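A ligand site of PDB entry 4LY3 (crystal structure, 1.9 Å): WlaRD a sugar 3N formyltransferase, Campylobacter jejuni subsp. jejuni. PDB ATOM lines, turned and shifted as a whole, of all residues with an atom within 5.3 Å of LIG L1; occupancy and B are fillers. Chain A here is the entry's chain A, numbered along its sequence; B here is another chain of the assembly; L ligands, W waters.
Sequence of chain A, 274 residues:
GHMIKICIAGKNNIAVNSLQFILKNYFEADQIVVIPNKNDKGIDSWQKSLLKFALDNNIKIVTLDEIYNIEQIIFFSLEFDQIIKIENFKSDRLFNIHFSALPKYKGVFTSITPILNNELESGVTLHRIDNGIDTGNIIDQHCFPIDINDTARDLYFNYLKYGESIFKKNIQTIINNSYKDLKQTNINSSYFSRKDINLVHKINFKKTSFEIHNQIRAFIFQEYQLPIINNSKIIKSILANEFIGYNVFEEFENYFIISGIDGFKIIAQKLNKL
Merely in contact with LIG L1: Ser 193 (3.3 Å), Ile 129 (3.4 Å), Ile 83 (3.5 Å), His 127 (3.5 Å), Ser 77 (3.5 Å), Asn 96 (3.6 Å), Asn 131 (3.8 Å), Val 108 (3.8 Å), Asp 81 (3.8 Å) and Ile 133 (3.9 Å).
Hydrophobic or aromatic side chains within 4 Å of LIG L1: Ile 83, Ile 84, Val 108, His 127, Ile 129 and Ile 133.
17 residues have an atom within 4 Å of LIG L1: Ser 77, Phe 80, Asp 81, Gln 82, Ile 83, Ile 84, Asn 96, Val 108, His 127, Ile 129, Asp 130, Asn 131, Gly 132, Ile 133, Asp 134, Ser 193 and Arg 194.
The nearest printed residue that does not touch LIG L1 is Tyr 191 (4.001 Å).
Water W1 lies within hydrogen-bond range of O6 of LIG L1 (2.8 Å), O of Gly 132 (2.9 Å), N of Asp 130 (3.0 Å) and N of Thr 135 (3.3 Å).
Water W3 lies within hydrogen-bond range of O2 of LIG L1, N of Lys 195, OG of Ser 193 and N of Arg 194.
Water W5 lies within hydrogen-bond range of OH of Tyr 191 (2.6 Å) and O1 of LIG L1 (2.9 Å).
Water W2 lies within hydrogen-bond range of the side-chain hydroxyl of Tyr 191 (2.5 Å) and an oxygen (O4) of LIG L1 (3.2 Å).
Water W4 lies within hydrogen-bond range of the side-chain carboxylate of Asp 134 (2.7 Å), a nitrogen (N3) of LG2 L2 (2.8 Å) and the backbone carbonyl oxygen of Gly 107 (3.1 Å).
N of Gly 132 lies within hydrogen-bond range of OD2 of Asp 130.
The side-chain carboxylate (OD2) of Asp 130 lies within hydrogen-bond range of the side-chain hydroxyl (OG1) of Thr 135 (2.6 Å).
OG1 of Thr 135 sits close to O of Gly 132, at 3.2 Å.
The side-chain carboxylate (OD2) of Asp 134 sits at hydrogen-bond distance from the backbone NH (N) of Gly 107.
The backbone NH of Phe 80 sits close to the side-chain hydroxyl of Ser 77, 3.5 Å away.
A ring nitrogen (NE2) of His 127 is in hydrogen-bond range of the side-chain amide oxygen (OD1) of Asn 96 (2.9 Å).
The side-chain amide nitrogen of Asn 96 sits at hydrogen-bond distance from the side-chain hydroxyl of Ser 77 (2.8 Å).
The backbone carbonyl oxygen (O) of Phe 192 sits at hydrogen-bond distance from the backbone NH (N) of Val 108.
The backbone carbonyl oxygen (O) of Asp 130 is in hydrogen-bond range of a nitrogen (N7) of LIG L1, at 2.8 Å.
A nitrogen (N1) of LIG L1 sits at hydrogen-bond distance from the backbone carbonyl oxygen of Gly 132 (2.8 Å).
The backbone carbonyl oxygen of Gln 82 lies within hydrogen-bond range of a nitrogen (N3) of LIG L1, 2.8 Å away.
The backbone NH (N) of Asp 134 sits at hydrogen-bond distance from an oxygen (O6) of LIG L1 (2.8 Å).
A nitrogen (N2) of LIG L1 lies within hydrogen-bond range of the backbone NH (N) of Ile 84.
A nitrogen (N7) of LIG L1 is in hydrogen-bond range of the backbone carbonyl oxygen (O) of Ile 84, at 2.8 Å.
The backbone NH of Arg 194 sits at hydrogen-bond distance from an oxygen (O1) of LIG L1, at 2.9 Å.
O2 of LIG L1 is in salt-bridge range of NH1 of Arg 194.
O of Phe 80 lies within hydrogen-bond range of N5 of LIG L1 (3.4 Å).
N of Phe 80 sits at hydrogen-bond distance from O12 of LG2 L2, at 3.1 Å.
The backbone carbonyl oxygen of Phe 80 lies within hydrogen-bond range of an oxygen (O12) of LG2 L2 (2.6 Å).
The backbone carbonyl oxygen (O) of Gly 107 sits at hydrogen-bond distance from an oxygen (O14) of LG2 L2 (2.8 Å).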
ATOM      1  N   SER A  77     -14.746 -23.583  27.987  1.00  0.00           N
ATOM      2  CA  SER A  77     -15.486 -23.021  26.859  1.00  0.00           C
ATOM      3  C   SER A  77     -15.735 -24.082  25.768  1.00  0.00           C
ATOM      4  O   SER A  77     -14.834 -24.782  25.309  1.00  0.00           O
ATOM      5  CB  SER A  77     -14.730 -21.830  26.238  1.00  0.00           C
ATOM      6  OG  SER A  77     -15.228 -21.554  24.926  1.00  0.00           O
ATOM      7  N   PHE A  80     -18.241 -21.118  23.241  1.00  0.00           N
ATOM      8  CA  PHE A  80     -18.670 -19.951  23.996  1.00  0.00           C
ATOM      9  C   PHE A  80     -18.460 -18.710  23.149  1.00  0.00           C
ATOM     10  O   PHE A  80     -17.508 -18.641  22.369  1.00  0.00           O
ATOM     11  CB  PHE A  80     -17.842 -19.895  25.281  1.00  0.00           C
ATOM     12  CG  PHE A  80     -18.213 -18.825  26.255  1.00  0.00           C
ATOM     13  CD1 PHE A  80     -17.229 -18.071  26.890  1.00  0.00           C
ATOM     14  CD2 PHE A  80     -19.535 -18.605  26.621  1.00  0.00           C
ATOM     15  CE1 PHE A  80     -17.551 -17.111  27.846  1.00  0.00           C
ATOM     16  CE2 PHE A  80     -19.878 -17.641  27.553  1.00  0.00           C
ATOM     17  CZ  PHE A  80     -18.879 -16.886  28.172  1.00  0.00           C
ATOM     18  N   ASP A  81     -19.303 -17.732  23.366  1.00  0.00           N
ATOM     19  CA  ASP A  81     -19.441 -16.557  22.504  1.00  0.00           C
ATOM     20  C   ASP A  81     -18.703 -15.323  22.992  1.00  0.00           C
ATOM     21  O   ASP A  81     -18.826 -14.311  22.370  1.00  0.00           O
ATOM     22  CB  ASP A  81     -20.908 -16.214  22.193  1.00  0.00           C
ATOM     23  CG  ASP A  81     -21.737 -15.719  23.407  1.00  0.00           C
ATOM     24  OD1 ASP A  81     -22.880 -15.226  23.234  1.00  0.00           O
ATOM     25  OD2 ASP A  81     -21.274 -15.714  24.538  1.00  0.00           O
ATOM     26  N   GLN A  82     -17.957 -15.402  24.070  1.00  0.00           N
ATOM     27  CA  GLN A  82     -17.228 -14.231  24.626  1.00  0.00           C
ATOM     28  C   GLN A  82     -15.740 -14.505  24.672  1.00  0.00           C
ATOM     29  O   GLN A  82     -15.328 -15.597  25.016  1.00  0.00           O
ATOM     30  CB  GLN A  82     -17.660 -13.961  26.047  1.00  0.00           C
ATOM     31  CG  GLN A  82     -19.109 -13.616  26.159  1.00  0.00           C
ATOM     32  CD  GLN A  82     -19.508 -13.075  27.516  1.00  0.00           C
ATOM     33  OE1 GLN A  82     -19.094 -11.975  27.878  1.00  0.00           O
ATOM     34  NE2 GLN A  82     -20.368 -13.806  28.252  1.00  0.00           N
ATOM     35  N   ILE A  83     -14.956 -13.502  24.291  1.00  0.00           N
ATOM     36  CA  ILE A  83     -13.495 -13.565  24.404  1.00  0.00           C
ATOM     37  C   ILE A  83     -13.149 -13.213  25.856  1.00  0.00           C
ATOM     38  O   ILE A  83     -13.466 -12.127  26.300  1.00  0.00           O
ATOM     39  CB  ILE A  83     -12.792 -12.508  23.542  1.00  0.00           C
ATOM     40  CG1 ILE A  83     -13.171 -12.651  22.076  1.00  0.00           C
ATOM     41  CG2 ILE A  83     -11.283 -12.649  23.678  1.00  0.00           C
ATOM     42  CD1 ILE A  83     -12.562 -13.872  21.463  1.00  0.00           C
ATOM     43  N   ILE A  84     -12.525 -14.097  26.595  1.00  0.00           N
ATOM     44  CA  ILE A  84     -12.255 -13.731  27.976  1.00  0.00           C
ATOM     45  C   ILE A  84     -10.850 -13.071  28.117  1.00  0.00           C
ATOM     46  O   ILE A  84     -10.052 -13.137  27.198  1.00  0.00           O
ATOM     47  CB  ILE A  84     -12.353 -14.951  28.912  1.00  0.00           C
ATOM     48  CG1 ILE A  84     -11.204 -15.894  28.651  1.00  0.00           C
ATOM     49  CG2 ILE A  84     -13.716 -15.637  28.824  1.00  0.00           C
ATOM     50  CD1 ILE A  84     -11.104 -16.993  29.646  1.00  0.00           C
ATOM     51  N   LYS A  85     -10.594 -12.477  29.287  1.00  0.00           N
ATOM     52  CA  LYS A  85      -9.314 -11.814  29.610  1.00  0.00           C
ATOM     53  C   LYS A  85      -8.862 -12.497  30.869  1.00  0.00           C
ATOM     54  O   LYS A  85      -9.591 -12.497  31.845  1.00  0.00           O
ATOM     55  CB  LYS A  85      -9.523 -10.350  29.861  1.00  0.00           C
ATOM     56  CG  LYS A  85     -10.146  -9.601  28.698  1.00  0.00           C
ATOM     57  CD  LYS A  85     -10.217  -8.165  29.090  1.00  0.00           C
ATOM     58  CE  LYS A  85     -10.827  -7.303  27.993  1.00  0.00           C
ATOM     59  NZ  LYS A  85     -12.263  -7.673  27.827  1.00  0.00           N
ATOM     60  N   ASN A  96     -10.524 -24.437  26.325  1.00  0.00           N
ATOM     61  CA  ASN A  96     -11.394 -24.241  25.170  1.00  0.00           C
ATOM     62  C   ASN A  96     -11.202 -25.403  24.237  1.00  0.00           C
ATOM     63  O   ASN A  96     -10.117 -25.977  24.166  1.00  0.00           O
ATOM     64  CB  ASN A  96     -11.087 -22.937  24.408  1.00  0.00           C
ATOM     65  CG  ASN A  96     -11.912 -22.788  23.132  1.00  0.00           C
ATOM     66  OD1 ASN A  96     -11.404 -22.676  21.985  1.00  0.00           O
ATOM     67  ND2 ASN A  96     -13.203 -22.704  23.330  1.00  0.00           N
ATOM     68  N   GLY A 107     -10.049 -18.186  14.864  1.00  0.00           N
ATOM     69  CA  GLY A 107     -11.159 -17.300  14.628  1.00  0.00           C
ATOM     70  C   GLY A 107     -12.433 -18.033  14.333  1.00  0.00           C
ATOM     71  O   GLY A 107     -12.698 -19.053  14.928  1.00  0.00           O
ATOM     72  N   VAL A 108     -13.241 -17.519  13.405  1.00  0.00           N
ATOM     73  CA  VAL A 108     -14.644 -17.878  13.309  1.00  0.00           C
ATOM     74  C   VAL A 108     -14.961 -18.596  11.968  1.00  0.00           C
ATOM     75  O   VAL A 108     -14.121 -18.752  11.037  1.00  0.00           O
ATOM     76  CB  VAL A 108     -15.548 -16.627  13.541  1.00  0.00           C
ATOM     77  CG1 VAL A 108     -15.239 -15.988  14.921  1.00  0.00           C
ATOM     78  CG2 VAL A 108     -15.328 -15.599  12.442  1.00  0.00           C
ATOM     79  N   HIS A 127      -7.206 -26.746  23.901  1.00  0.00           N
ATOM     80  CA  HIS A 127      -6.080 -25.870  24.271  1.00  0.00           C
ATOM     81  C   HIS A 127      -6.402 -25.058  25.495  1.00  0.00           C
ATOM     82  O   HIS A 127      -7.589 -24.876  25.830  1.00  0.00           O
ATOM     83  CB  HIS A 127      -5.725 -24.968  23.092  1.00  0.00           C
ATOM     84  CG  HIS A 127      -6.802 -24.023  22.691  1.00  0.00           C
ATOM     85  ND1 HIS A 127      -6.855 -22.740  23.173  1.00  0.00           N
ATOM     86  CD2 HIS A 127      -7.882 -24.182  21.901  1.00  0.00           C
ATOM     87  CE1 HIS A 127      -7.927 -22.133  22.691  1.00  0.00           C
ATOM     88  NE2 HIS A 127      -8.540 -22.978  21.877  1.00  0.00           N
ATOM     89  N   ILE A 129      -6.723 -21.512  27.303  1.00  0.00           N
ATOM     90  CA  ILE A 129      -7.108 -20.161  26.843  1.00  0.00           C
ATOM     91  C   ILE A 129      -6.053 -19.163  27.299  1.00  0.00           C
ATOM     92  O   ILE A 129      -5.783 -19.105  28.525  1.00  0.00           O
ATOM     93  CB  ILE A 129      -8.460 -19.740  27.408  1.00  0.00           C
ATOM     94  CG1 ILE A 129      -9.562 -20.699  26.882  1.00  0.00           C
ATOM     95  CG2 ILE A 129      -8.698 -18.274  27.080  1.00  0.00           C
ATOM     96  CD1 ILE A 129     -10.910 -20.454  27.485  1.00  0.00           C
ATOM     97  N   ASP A 130      -5.521 -18.341  26.383  1.00  0.00           N
ATOM     98  CA  ASP A 130      -4.768 -17.172  26.806  1.00  0.00           C
ATOM     99  C   ASP A 130      -5.514 -15.975  26.266  1.00  0.00           C
ATOM    100  O   ASP A 130      -6.681 -16.127  25.856  1.00  0.00           O
ATOM    101  CB  ASP A 130      -3.297 -17.267  26.422  1.00  0.00           C
ATOM    102  CG  ASP A 130      -3.093 -17.349  24.878  1.00  0.00           C
ATOM    103  OD1 ASP A 130      -2.042 -17.827  24.472  1.00  0.00           O
ATOM    104  OD2 ASP A 130      -3.984 -16.923  24.137  1.00  0.00           O
ATOM    105  N   ASN A 131      -4.921 -14.797  26.253  1.00  0.00           N
ATOM    106  CA  ASN A 131      -5.692 -13.623  25.897  1.00  0.00           C
ATOM    107  C   ASN A 131      -5.883 -13.465  24.411  1.00  0.00           C
ATOM    108  O   ASN A 131      -6.586 -12.537  24.035  1.00  0.00           O
ATOM    109  CB  ASN A 131      -5.075 -12.320  26.441  1.00  0.00           C
ATOM    110  CG  ASN A 131      -5.354 -12.134  27.945  1.00  0.00           C
ATOM    111  OD1 ASN A 131      -6.375 -12.589  28.440  1.00  0.00           O
ATOM    112  ND2 ASN A 131      -4.450 -11.441  28.664  1.00  0.00           N
ATOM    113  N   GLY A 132      -5.230 -14.255  23.598  1.00  0.00           N
ATOM    114  CA  GLY A 132      -5.487 -14.159  22.162  1.00  0.00           C
ATOM    115  C   GLY A 132      -6.620 -15.104  21.768  1.00  0.00           C
ATOM    116  O   GLY A 132      -7.022 -15.999  22.564  1.00  0.00           O
ATOM    117  N   ILE A 133      -7.064 -14.936  20.536  1.00  0.00           N
ATOM    118  CA  ILE A 133      -8.137 -15.781  20.024  1.00  0.00           C
ATOM    119  C   ILE A 133      -7.531 -17.077  19.497  1.00  0.00           C
ATOM    120  O   ILE A 133      -6.850 -17.104  18.455  1.00  0.00           O
ATOM    121  CB  ILE A 133      -8.911 -15.044  18.927  1.00  0.00           C
ATOM    122  CG1 ILE A 133      -9.624 -13.841  19.480  1.00  0.00           C
ATOM    123  CG2 ILE A 133      -9.939 -15.994  18.287  1.00  0.00           C
ATOM    124  CD1 ILE A 133      -9.964 -12.763  18.462  1.00  0.00           C
ATOM    125  N   ASP A 134      -7.799 -18.172  20.195  1.00  0.00           N
ATOM    126  CA  ASP A 134      -7.416 -19.538  19.794  1.00  0.00           C
ATOM    127  C   ASP A 134      -5.931 -19.739  19.691  1.00  0.00           C
ATOM    128  O   ASP A 134      -5.442 -20.597  18.920  1.00  0.00           O
ATOM    129  CB  ASP A 134      -8.084 -19.966  18.478  1.00  0.00           C
ATOM    130  CG  ASP A 134      -9.590 -19.807  18.504  1.00  0.00           C
ATOM    131  OD1 ASP A 134     -10.204 -20.076  19.560  1.00  0.00           O
ATOM    132  OD2 ASP A 134     -10.156 -19.376  17.470  1.00  0.00           O
ATOM    133  N   THR A 135      -5.210 -18.906  20.455  1.00  0.00           N
ATOM    134  CA  THR A 135      -3.753 -18.889  20.477  1.00  0.00           C
ATOM    135  C   THR A 135      -3.036 -19.739  21.490  1.00  0.00           C
ATOM    136  O   THR A 135      -1.832 -19.921  21.358  1.00  0.00           O
ATOM    137  CB  THR A 135      -3.282 -17.456  20.655  1.00  0.00           C
ATOM    138  OG1 THR A 135      -4.109 -16.749  21.596  1.00  0.00           O
ATOM    139  CG2 THR A 135      -3.426 -16.729  19.255  1.00  0.00           C
ATOM    140  N   TYR A 191      -5.930 -17.181  10.544  1.00  0.00           N
ATOM    141  CA  TYR A 191      -7.016 -16.635  11.280  1.00  0.00           C
ATOM    142  C   TYR A 191      -8.022 -16.062  10.371  1.00  0.00           C
ATOM    143  O   TYR A 191      -7.618 -15.384   9.415  1.00  0.00           O
ATOM    144  CB  TYR A 191      -6.494 -15.541  12.210  1.00  0.00           C
ATOM    145  CG  TYR A 191      -7.519 -14.652  12.901  1.00  0.00           C
ATOM    146  CD1 TYR A 191      -8.178 -15.084  14.028  1.00  0.00           C
ATOM    147  CD2 TYR A 191      -7.771 -13.355  12.466  1.00  0.00           C
ATOM    148  CE1 TYR A 191      -9.091 -14.310  14.707  1.00  0.00           C
ATOM    149  CE2 TYR A 191      -8.724 -12.564  13.104  1.00  0.00           C
ATOM    150  CZ  TYR A 191      -9.342 -13.022  14.267  1.00  0.00           C
ATOM    151  OH  TYR A 191     -10.291 -12.325  14.967  1.00  0.00           O
ATOM    152  N   PHE A 192      -9.304 -16.250  10.703  1.00  0.00           N
ATOM    153  CA  PHE A 192     -10.377 -15.552   9.979  1.00  0.00           C
ATOM    154  C   PHE A 192     -11.339 -14.921  10.921  1.00  0.00           C
ATOM    155  O   PHE A 192     -11.743 -15.558  11.889  1.00  0.00           O
ATOM    156  CB  PHE A 192     -11.123 -16.529   9.022  1.00  0.00           C
ATOM    157  CG  PHE A 192     -10.227 -17.043   7.937  1.00  0.00           C
ATOM    158  CD1 PHE A 192     -10.150 -16.362   6.737  1.00  0.00           C
ATOM    159  CD2 PHE A 192      -9.359 -18.097   8.164  1.00  0.00           C
ATOM    160  CE1 PHE A 192      -9.262 -16.759   5.763  1.00  0.00           C
ATOM    161  CE2 PHE A 192      -8.472 -18.494   7.190  1.00  0.00           C
ATOM    162  CZ  PHE A 192      -8.423 -17.821   5.984  1.00  0.00           C
ATOM    163  N   SER A 193     -11.701 -13.671  10.633  1.00  0.00           N
ATOM    164  CA  SER A 193     -12.681 -12.968  11.460  1.00  0.00           C
ATOM    165  C   SER A 193     -13.918 -12.745  10.604  1.00  0.00           C
ATOM    166  O   SER A 193     -13.924 -13.093   9.437  1.00  0.00           O
ATOM    167  CB  SER A 193     -12.085 -11.677  12.003  1.00  0.00           C
ATOM    168  OG  SER A 193     -12.094 -10.624  11.056  1.00  0.00           O
ATOM    169  N   ARG A 194     -14.980 -12.217  11.212  1.00  0.00           N
ATOM    170  CA  ARG A 194     -16.309 -12.160  10.600  1.00  0.00           C
ATOM    171  C   ARG A 194     -16.258 -11.380   9.331  1.00  0.00           C
ATOM    172  O   ARG A 194     -16.771 -11.803   8.331  1.00  0.00           O
ATOM    173  CB  ARG A 194     -17.321 -11.516  11.540  1.00  0.00           C
ATOM    174  CG  ARG A 194     -17.674 -12.498  12.625  1.00  0.00           C
ATOM    175  CD  ARG A 194     -18.940 -12.167  13.399  1.00  0.00           C
ATOM    176  NE  ARG A 194     -19.046 -13.180  14.460  1.00  0.00           N
ATOM    177  CZ  ARG A 194     -18.605 -13.026  15.708  1.00  0.00           C
ATOM    178  NH1 ARG A 194     -18.100 -11.858  16.132  1.00  0.00           N
ATOM    179  NH2 ARG A 194     -18.728 -14.047  16.561  1.00  0.00           N
ATOM    180  N   LYS A 195     -15.547 -10.274   9.383  1.00  0.00           N
ATOM    181  CA  LYS A 195     -15.419  -9.426   8.210  1.00  0.00           C
ATOM    182  C   LYS A 195     -14.687 -10.130   7.077  1.00  0.00           C
ATOM    183  O   LYS A 195     -14.707  -9.658   5.976  1.00  0.00           O
ATOM    184  CB  LYS A 195     -14.685  -8.129   8.560  1.00  0.00           C
ATOM    185  CG  LYS A 195     -13.177  -8.302   8.436  1.00  0.00           C
ATOM    186  CD  LYS A 195     -12.412  -7.094   8.958  1.00  0.00           C
ATOM    187  CE  LYS A 195     -11.064  -7.489   9.525  1.00  0.00           C
ATOM    188  NZ  LYS A 195     -10.133  -8.000   8.469  1.00  0.00           N
ATOM    189  N   LYS B 206      -5.511  -7.815  10.605  1.00  0.00           N
ATOM    190  CA  LYS B 206      -6.276  -8.672  11.497  1.00  0.00           C
ATOM    191  C   LYS B 206      -6.134 -10.140  11.083  1.00  0.00           C
ATOM    192  O   LYS B 206      -7.116 -10.846  10.703  1.00  0.00           O
ATOM    193  CB  LYS B 206      -7.707  -8.196  11.530  1.00  0.00           C
ATOM    194  CG  LYS B 206      -7.882  -6.819  12.104  1.00  0.00           C
ATOM    195  CD  LYS B 206      -7.924  -6.864  13.621  1.00  0.00           C
ATOM    196  CE  LYS B 206      -7.895  -5.488  14.280  1.00  0.00           C
ATOM    197  NZ  LYS B 206      -9.249  -4.870  14.375  1.00  0.00           N
HETATM  198  N1  LIG L   1      -9.173 -16.956  24.007  1.00  0.00           N
HETATM  199  C1  LIG L   1      -9.866 -16.058  24.722  1.00  0.00           C
HETATM  200  N2  LIG L   1     -11.195 -16.183  24.967  1.00  0.00           N
HETATM  201  C2  LIG L   1     -11.845 -17.228  24.410  1.00  0.00           C
HETATM  202  C3  LIG L   1     -11.165 -18.141  23.596  1.00  0.00           C
HETATM  203  C4  LIG L   1      -9.800 -17.980  23.387  1.00  0.00           C
HETATM  204  N3  LIG L   1     -13.152 -17.308  24.644  1.00  0.00           N
HETATM  205  C5  LIG L   1     -13.886 -18.425  23.997  1.00  0.00           C
HETATM  206  C6  LIG L   1     -13.234 -18.994  22.714  1.00  0.00           C
HETATM  207  N4  LIG L   1     -11.826 -19.160  22.969  1.00  0.00           N
HETATM  208  C7  LIG L   1     -13.294 -18.220  21.386  1.00  0.00           C
HETATM  209  N5  LIG L   1     -14.526 -17.509  21.133  1.00  0.00           N
HETATM  210  C8  LIG L   1     -14.679 -16.480  20.269  1.00  0.00           C
HETATM  211  C9  LIG L   1     -15.730 -15.604  20.554  1.00  0.00           C
HETATM  212  C10 LIG L   1     -15.976 -14.474  19.787  1.00  0.00           C
HETATM  213  C11 LIG L   1     -15.142 -14.170  18.702  1.00  0.00           C
HETATM  214  C12 LIG L   1     -14.084 -15.034  18.417  1.00  0.00           C
HETATM  215  C13 LIG L   1     -13.831 -16.169  19.190  1.00  0.00           C
HETATM  216  C14 LIG L   1     -15.430 -12.901  17.966  1.00  0.00           C
HETATM  217  N6  LIG L   1     -14.639 -12.428  17.004  1.00  0.00           N
HETATM  218  C15 LIG L   1     -14.821 -11.181  16.281  1.00  0.00           C
HETATM  219  C16 LIG L   1     -15.008 -11.264  14.785  1.00  0.00           C
HETATM  220  O1  LIG L   1     -14.565 -12.246  14.132  1.00  0.00           O
HETATM  221  O2  LIG L   1     -15.608 -10.302  14.262  1.00  0.00           O
HETATM  222  C17 LIG L   1     -13.494 -10.442  16.450  1.00  0.00           C
HETATM  223  C18 LIG L   1     -13.371  -9.892  17.866  1.00  0.00           C
HETATM  224  C19 LIG L   1     -12.074  -9.137  18.098  1.00  0.00           C
HETATM  225  O3  LIG L   1     -11.857  -8.841  19.304  1.00  0.00           O
HETATM  226  O4  LIG L   1     -11.306  -8.840  17.139  1.00  0.00           O
HETATM  227  O5  LIG L   1     -16.401 -12.265  18.376  1.00  0.00           O
HETATM  228  O6  LIG L   1      -9.001 -18.809  22.663  1.00  0.00           O
HETATM  229  N7  LIG L   1      -9.161 -15.063  25.315  1.00  0.00           N
HETATM  230  O1  LG2 L   2     -24.555 -17.116   9.383  1.00  0.00           O
HETATM  231  C1  LG2 L   2     -23.912 -18.198   9.496  1.00  0.00           C
HETATM  232  N1  LG2 L   2     -23.734 -19.003   8.429  1.00  0.00           N
HETATM  233  C2  LG2 L   2     -23.093 -20.177   8.598  1.00  0.00           C
HETATM  234  O2  LG2 L   2     -22.921 -20.871   7.533  1.00  0.00           O
HETATM  235  C3  LG2 L   2     -23.407 -18.600  10.725  1.00  0.00           C
HETATM  236  C4  LG2 L   2     -23.671 -17.682  11.906  1.00  0.00           C
HETATM  237  C5  LG2 L   2     -22.806 -19.740  10.847  1.00  0.00           C
HETATM  238  N2  LG2 L   2     -22.636 -20.524   9.804  1.00  0.00           N
HETATM  239  C6  LG2 L   2     -21.911 -21.796   9.972  1.00  0.00           C
HETATM  240  O3  LG2 L   2     -22.179 -22.334  11.263  1.00  0.00           O
HETATM  241  C7  LG2 L   2     -20.407 -21.582   9.877  1.00  0.00           C
HETATM  242  C8  LG2 L   2     -19.876 -21.824  11.295  1.00  0.00           C
HETATM  243  O4  LG2 L   2     -18.602 -22.438  11.313  1.00  0.00           O
HETATM  244  C9  LG2 L   2     -20.974 -22.664  11.926  1.00  0.00           C
HETATM  245  C10 LG2 L   2     -21.154 -22.422  13.422  1.00  0.00           C
HETATM  246  O5  LG2 L   2     -21.546 -21.077  13.614  1.00  0.00           O
HETATM  247  P1  LG2 L   2     -21.272 -20.328  14.996  1.00  0.00           P
HETATM  248  O6  LG2 L   2     -21.808 -21.291  16.036  1.00  0.00           O
HETATM  249  O7  LG2 L   2     -21.726 -18.903  14.807  1.00  0.00           O
HETATM  250  O8  LG2 L   2     -19.725 -20.553  15.299  1.00  0.00           O
HETATM  251  P2  LG2 L   2     -18.387 -20.299  14.421  1.00  0.00           P
HETATM  252  O9  LG2 L   2     -17.987 -21.572  13.623  1.00  0.00           O
HETATM  253  O10 LG2 L   2     -18.375 -18.903  13.918  1.00  0.00           O
HETATM  254  O11 LG2 L   2     -17.484 -20.339  15.751  1.00  0.00           O
HETATM  255  O12 LG2 L   2     -17.263 -20.346  20.365  1.00  0.00           O
HETATM  256  C11 LG2 L   2     -17.150 -19.482  19.221  1.00  0.00           C
HETATM  257  C12 LG2 L   2     -18.424 -19.361  18.386  1.00  0.00           C
HETATM  258  O13 LG2 L   2     -18.120 -18.553  17.234  1.00  0.00           O
HETATM  259  C13 LG2 L   2     -19.650 -18.796  19.078  1.00  0.00           C
HETATM  260  C14 LG2 L   2     -16.127 -20.185  18.378  1.00  0.00           C
HETATM  261  N3  LG2 L   2     -14.931 -20.472  19.151  1.00  0.00           N
HETATM  262  C15 LG2 L   2     -15.800 -19.331  17.146  1.00  0.00           C
HETATM  263  O14 LG2 L   2     -14.863 -20.058  16.335  1.00  0.00           O
HETATM  264  C16 LG2 L   2     -17.109 -19.084  16.376  1.00  0.00           C
HETATM  265  O   HOH W   1      -6.359 -18.656  23.558  1.00  0.00           O
HETATM  266  O   HOH W   2     -10.263  -9.881  14.286  1.00  0.00           O
HETATM  267  O   HOH W   3     -14.846  -8.890  11.917  1.00  0.00           O
HETATM  268  O   HOH W   4     -12.776 -19.141  18.027  1.00  0.00           O
HETATM  269  O   HOH W   5     -12.453 -13.764  15.426  1.00  0.00           O
